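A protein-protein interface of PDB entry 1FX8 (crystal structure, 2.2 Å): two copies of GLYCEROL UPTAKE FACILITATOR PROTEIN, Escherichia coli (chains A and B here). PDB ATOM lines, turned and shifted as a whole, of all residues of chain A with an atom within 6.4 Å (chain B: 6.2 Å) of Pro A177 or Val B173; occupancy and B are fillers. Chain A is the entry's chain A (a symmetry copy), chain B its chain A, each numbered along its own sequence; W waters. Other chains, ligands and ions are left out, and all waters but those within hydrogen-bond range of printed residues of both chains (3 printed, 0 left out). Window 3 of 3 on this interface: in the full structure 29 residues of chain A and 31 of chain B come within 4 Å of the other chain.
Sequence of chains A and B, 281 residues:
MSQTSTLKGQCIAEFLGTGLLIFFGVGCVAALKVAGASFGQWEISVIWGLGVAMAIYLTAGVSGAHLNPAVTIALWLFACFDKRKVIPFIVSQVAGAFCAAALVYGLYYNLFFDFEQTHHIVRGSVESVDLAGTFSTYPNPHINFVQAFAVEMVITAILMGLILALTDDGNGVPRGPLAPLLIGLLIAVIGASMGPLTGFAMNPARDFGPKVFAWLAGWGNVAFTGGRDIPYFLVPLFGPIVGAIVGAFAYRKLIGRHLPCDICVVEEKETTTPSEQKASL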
ATOM      1  N   TYR A  57     -17.737 -20.645   1.544  1.00  0.00           N
ATOM      2  CA  TYR A  57     -16.943 -21.411   0.588  1.00  0.00           C
ATOM      3  C   TYR A  57     -17.622 -22.722   0.216  1.00  0.00           C
ATOM      4  O   TYR A  57     -17.499 -23.214  -0.914  1.00  0.00           O
ATOM      5  CB  TYR A  57     -15.558 -21.729   1.167  1.00  0.00           C
ATOM      6  CG  TYR A  57     -14.566 -20.593   1.067  1.00  0.00           C
ATOM      7  CD1 TYR A  57     -14.241 -20.031  -0.176  1.00  0.00           C
ATOM      8  CD2 TYR A  57     -13.951 -20.075   2.213  1.00  0.00           C
ATOM      9  CE1 TYR A  57     -13.325 -18.977  -0.275  1.00  0.00           C
ATOM     10  CE2 TYR A  57     -13.036 -19.023   2.126  1.00  0.00           C
ATOM     11  CZ  TYR A  57     -12.731 -18.481   0.879  1.00  0.00           C
ATOM     12  OH  TYR A  57     -11.847 -17.431   0.791  1.00  0.00           O
ATOM     13  N   GLY A  61     -21.103 -21.774  -4.318  1.00  0.00           N
ATOM     14  CA  GLY A  61     -21.261 -22.344  -5.644  1.00  0.00           C
ATOM     15  C   GLY A  61     -22.617 -22.951  -5.946  1.00  0.00           C
ATOM     16  O   GLY A  61     -22.955 -23.148  -7.111  1.00  0.00           O
ATOM     17  N   ARG A 175     -12.111  -9.261  -5.896  1.00  0.00           N
ATOM     18  CA  ARG A 175     -11.510 -10.083  -4.847  1.00  0.00           C
ATOM     19  C   ARG A 175     -11.409 -11.544  -5.234  1.00  0.00           C
ATOM     20  O   ARG A 175     -10.562 -12.267  -4.714  1.00  0.00           O
ATOM     21  CB  ARG A 175     -12.301  -9.995  -3.535  1.00  0.00           C
ATOM     22  CG  ARG A 175     -12.172  -8.684  -2.783  1.00  0.00           C
ATOM     23  CD  ARG A 175     -13.210  -7.707  -3.260  1.00  0.00           C
ATOM     24  NE  ARG A 175     -12.599  -6.483  -3.742  1.00  0.00           N
ATOM     25  CZ  ARG A 175     -13.232  -5.575  -4.470  1.00  0.00           C
ATOM     26  NH1 ARG A 175     -14.503  -5.758  -4.801  1.00  0.00           N
ATOM     27  NH2 ARG A 175     -12.585  -4.494  -4.873  1.00  0.00           N
ATOM     28  N   GLY A 176     -12.279 -11.985  -6.135  1.00  0.00           N
ATOM     29  CA  GLY A 176     -12.249 -13.376  -6.537  1.00  0.00           C
ATOM     30  C   GLY A 176     -12.443 -14.312  -5.352  1.00  0.00           C
ATOM     31  O   GLY A 176     -13.374 -14.131  -4.564  1.00  0.00           O
ATOM     32  N   PRO A 177     -11.569 -15.314  -5.186  1.00  0.00           N
ATOM     33  CA  PRO A 177     -11.669 -16.272  -4.081  1.00  0.00           C
ATOM     34  C   PRO A 177     -11.440 -15.701  -2.677  1.00  0.00           C
ATOM     35  O   PRO A 177     -11.657 -16.395  -1.688  1.00  0.00           O
ATOM     36  CB  PRO A 177     -10.636 -17.332  -4.459  1.00  0.00           C
ATOM     37  CG  PRO A 177      -9.574 -16.524  -5.137  1.00  0.00           C
ATOM     38  CD  PRO A 177     -10.386 -15.597  -6.021  1.00  0.00           C
ATOM     39  N   LEU A 178     -11.013 -14.444  -2.592  1.00  0.00           N
ATOM     40  CA  LEU A 178     -10.763 -13.787  -1.309  1.00  0.00           C
ATOM     41  C   LEU A 178     -12.031 -13.259  -0.644  1.00  0.00           C
ATOM     42  O   LEU A 178     -12.062 -13.049   0.568  1.00  0.00           O
ATOM     43  CB  LEU A 178      -9.816 -12.598  -1.491  1.00  0.00           C
ATOM     44  CG  LEU A 178      -8.298 -12.751  -1.435  1.00  0.00           C
ATOM     45  CD1 LEU A 178      -7.662 -11.405  -1.758  1.00  0.00           C
ATOM     46  CD2 LEU A 178      -7.864 -13.228  -0.053  1.00  0.00           C
ATOM     47  N   ALA A 179     -13.062 -13.027  -1.451  1.00  0.00           N
ATOM     48  CA  ALA A 179     -14.326 -12.476  -0.973  1.00  0.00           C
ATOM     49  C   ALA A 179     -14.899 -13.106   0.304  1.00  0.00           C
ATOM     50  O   ALA A 179     -15.171 -12.398   1.274  1.00  0.00           O
ATOM     51  CB  ALA A 179     -15.363 -12.517  -2.099  1.00  0.00           C
ATOM     52  N   PRO A 180     -15.103 -14.435   0.318  1.00  0.00           N
ATOM     53  CA  PRO A 180     -15.651 -15.085   1.516  1.00  0.00           C
ATOM     54  C   PRO A 180     -14.812 -14.807   2.759  1.00  0.00           C
ATOM     55  O   PRO A 180     -15.349 -14.441   3.803  1.00  0.00           O
ATOM     56  CB  PRO A 180     -15.656 -16.562   1.133  1.00  0.00           C
ATOM     57  CG  PRO A 180     -15.885 -16.514  -0.352  1.00  0.00           C
ATOM     58  CD  PRO A 180     -14.935 -15.416  -0.771  1.00  0.00           C
ATOM     59  N   LEU A 181     -13.497 -14.972   2.636  1.00  0.00           N
ATOM     60  CA  LEU A 181     -12.583 -14.730   3.754  1.00  0.00           C
ATOM     61  C   LEU A 181     -12.738 -13.306   4.265  1.00  0.00           C
ATOM     62  O   LEU A 181     -12.843 -13.080   5.469  1.00  0.00           O
ATOM     63  CB  LEU A 181     -11.129 -14.952   3.328  1.00  0.00           C
ATOM     64  CG  LEU A 181     -10.062 -14.587   4.375  1.00  0.00           C
ATOM     65  CD1 LEU A 181     -10.149 -15.550   5.558  1.00  0.00           C
ATOM     66  CD2 LEU A 181      -8.669 -14.652   3.754  1.00  0.00           C
ATOM     67  N   ASP B 169     -12.630 -27.113  -7.658  1.00  0.00           N
ATOM     68  CA  ASP B 169     -12.671 -25.978  -8.575  1.00  0.00           C
ATOM     69  C   ASP B 169     -13.994 -25.761  -9.304  1.00  0.00           C
ATOM     70  O   ASP B 169     -14.192 -24.729  -9.943  1.00  0.00           O
ATOM     71  CB  ASP B 169     -11.528 -26.073  -9.584  1.00  0.00           C
ATOM     72  CG  ASP B 169     -10.181 -25.746  -8.965  1.00  0.00           C
ATOM     73  OD1 ASP B 169     -10.098 -24.749  -8.212  1.00  0.00           O
ATOM     74  OD2 ASP B 169      -9.200 -26.473  -9.234  1.00  0.00           O
ATOM     75  N   ASN B 171     -16.684 -25.562  -7.711  1.00  0.00           N
ATOM     76  CA  ASN B 171     -17.523 -24.972  -6.675  1.00  0.00           C
ATOM     77  C   ASN B 171     -17.170 -23.507  -6.469  1.00  0.00           C
ATOM     78  O   ASN B 171     -16.241 -23.191  -5.731  1.00  0.00           O
ATOM     79  CB  ASN B 171     -17.325 -25.718  -5.354  1.00  0.00           C
ATOM     80  CG  ASN B 171     -18.345 -25.327  -4.305  1.00  0.00           C
ATOM     81  OD1 ASN B 171     -18.758 -24.169  -4.220  1.00  0.00           O
ATOM     82  ND2 ASN B 171     -18.750 -26.291  -3.492  1.00  0.00           N
ATOM     83  N   GLY B 172     -17.915 -22.614  -7.108  1.00  0.00           N
ATOM     84  CA  GLY B 172     -17.634 -21.200  -6.959  1.00  0.00           C
ATOM     85  C   GLY B 172     -16.295 -20.831  -7.572  1.00  0.00           C
ATOM     86  O   GLY B 172     -15.773 -21.562  -8.414  1.00  0.00           O
ATOM     87  N   VAL B 173     -15.737 -19.702  -7.151  1.00  0.00           N
ATOM     88  CA  VAL B 173     -14.458 -19.244  -7.676  1.00  0.00           C
ATOM     89  C   VAL B 173     -13.307 -20.049  -7.083  1.00  0.00           C
ATOM     90  O   VAL B 173     -13.161 -20.136  -5.862  1.00  0.00           O
ATOM     91  CB  VAL B 173     -14.236 -17.747  -7.371  1.00  0.00           C
ATOM     92  CG1 VAL B 173     -12.928 -17.275  -7.978  1.00  0.00           C
ATOM     93  CG2 VAL B 173     -15.395 -16.932  -7.920  1.00  0.00           C
ATOM     94  N   PRO B 174     -12.476 -20.655  -7.949  1.00  0.00           N
ATOM     95  CA  PRO B 174     -11.323 -21.464  -7.525  1.00  0.00           C
ATOM     96  C   PRO B 174     -10.427 -20.708  -6.541  1.00  0.00           C
ATOM     97  O   PRO B 174     -10.151 -19.522  -6.739  1.00  0.00           O
ATOM     98  CB  PRO B 174     -10.609 -21.757  -8.843  1.00  0.00           C
ATOM     99  CG  PRO B 174     -11.739 -21.797  -9.837  1.00  0.00           C
ATOM    100  CD  PRO B 174     -12.579 -20.612  -9.420  1.00  0.00           C
ATOM    101  N   ARG B 175      -9.973 -21.392  -5.490  1.00  0.00           N
ATOM    102  CA  ARG B 175      -9.114 -20.759  -4.491  1.00  0.00           C
ATOM    103  C   ARG B 175      -7.668 -20.672  -4.932  1.00  0.00           C
ATOM    104  O   ARG B 175      -6.927 -19.809  -4.465  1.00  0.00           O
ATOM    105  CB  ARG B 175      -9.156 -21.507  -3.152  1.00  0.00           C
ATOM    106  CG  ARG B 175     -10.440 -21.352  -2.359  1.00  0.00           C
ATOM    107  CD  ARG B 175     -11.433 -22.404  -2.767  1.00  0.00           C
ATOM    108  NE  ARG B 175     -12.674 -21.808  -3.225  1.00  0.00           N
ATOM    109  CZ  ARG B 175     -13.607 -22.462  -3.900  1.00  0.00           C
ATOM    110  NH1 ARG B 175     -13.435 -23.744  -4.196  1.00  0.00           N
ATOM    111  NH2 ARG B 175     -14.701 -21.827  -4.286  1.00  0.00           N
ATOM    112  N   GLY B 176      -7.259 -21.570  -5.819  1.00  0.00           N
ATOM    113  CA  GLY B 176      -5.882 -21.556  -6.270  1.00  0.00           C
ATOM    114  C   GLY B 176      -4.906 -21.712  -5.113  1.00  0.00           C
ATOM    115  O   GLY B 176      -5.059 -22.617  -4.289  1.00  0.00           O
ATOM    116  N   LEU B 178      -4.677 -20.194  -2.407  1.00  0.00           N
ATOM    117  CA  LEU B 178      -5.289 -19.901  -1.110  1.00  0.00           C
ATOM    118  C   LEU B 178      -5.793 -21.147  -0.387  1.00  0.00           C
ATOM    119  O   LEU B 178      -5.961 -21.138   0.833  1.00  0.00           O
ATOM    120  CB  LEU B 178      -6.483 -18.960  -1.281  1.00  0.00           C
ATOM    121  CG  LEU B 178      -6.328 -17.441  -1.279  1.00  0.00           C
ATOM    122  CD1 LEU B 178      -7.685 -16.814  -1.576  1.00  0.00           C
ATOM    123  CD2 LEU B 178      -5.804 -16.963   0.071  1.00  0.00           C
ATOM    124  N   LEU B 182      -6.565 -21.743   3.656  1.00  0.00           N
ATOM    125  CA  LEU B 182      -7.951 -21.875   4.092  1.00  0.00           C
ATOM    126  C   LEU B 182      -8.176 -23.186   4.848  1.00  0.00           C
ATOM    127  O   LEU B 182      -8.958 -23.235   5.795  1.00  0.00           O
ATOM    128  CB  LEU B 182      -8.906 -21.762   2.888  1.00  0.00           C
ATOM    129  CG  LEU B 182      -8.838 -20.409   2.152  1.00  0.00           C
ATOM    130  CD1 LEU B 182      -9.747 -20.414   0.944  1.00  0.00           C
ATOM    131  CD2 LEU B 182      -9.234 -19.280   3.102  1.00  0.00           C
HETATM  132  O   HOH W   1     -18.071 -21.728  -3.136  1.00  0.00           O
HETATM  133  O   HOH W   2     -20.124 -23.195  -9.028  1.00  0.00           O
HETATM  134  O   HOH W   3     -21.091 -24.570  -3.500  1.00  0.00           O
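OD1 of Asn B171 is in hydrogen-bond range of N of Gly A61, at 3.4 Å.
The side-chain hydroxyl of Tyr A57 is in hydrogen-bond range of the backbone NH of Leu A181 (3.5 Å). The guanidinium group of Arg B175 is in hydrogen-bond range of the backbone carbonyl oxygen of Asn B171 (2.5 Å). The backbone carbonyl oxygen (O) of Val B173 sits at hydrogen-bond distance from the guanidinium group (NH2) of Arg B175 (2.8 Å). O of Pro A177 is in hydrogen-bond range of OH of Tyr A57 (2.7 Å).
Tyr A57 touches Asn B171. Tyr A57 touches Arg B175. Leu B182 touches Tyr A57. N of Gly B172 touches CA of Gly A61 (3.7 Å). C of Gly A176 touches CG1 of Val B173 (3.99 Å). Pro A177 touches Val B173. O of Pro B174 touches CB of Pro A177 (3.2 Å). Pro A177 touches Arg B175 (CB to CA, 3.7 Å). O of Pro A177 touches CD1 of Leu B178 (3.996 Å). Leu B178 touches Leu A178 (CD1 to CD2, 3.9 Å).
Of the printed residues of chain B, Pro A177 touches Val B173, Pro B174, Arg B175 and Leu B178. Of the printed residues of chain A, Asn B171 touches Tyr A57 (3.7 Å) and Gly A61 (3.4 Å). Printed residues of chain B within 4 Å of Tyr A57: Asn B171, Arg B175 and Leu B182. The nearest printed residue of chain B that does not touch Pro A177 is Leu B182 (5.2 Å).
Hydrophobic or aromatic side chains of chain A that line the printed part of chain B: Tyr A57, Pro A177 and Leu A178. Along chain A the printed residues that touch a printed residue of chain B span positions 57 to 178. Among the printed residues, 11 pairs touch across the chains. Among the printed residues, no Asp or Glu carboxylate lies within 4 Å of a Lys or Arg side-chain nitrogen of the other chain.
Leu B178 touches its own counterpart, Leu A178. Positions printed for both chains: 175, 176 and 178.
Water W3 bridges OD1 of Asn B171 (2.5 Å) and N of Gly A61 (2.9 Å). Water W1 lies within hydrogen-bond range of the backbone carbonyl oxygen of Tyr A57, the side-chain amide oxygen of Asn B171 and the backbone NH of Gly A61. Water W2 lies within hydrogen-bond range of N of Gly B172 and O of Gly A61.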
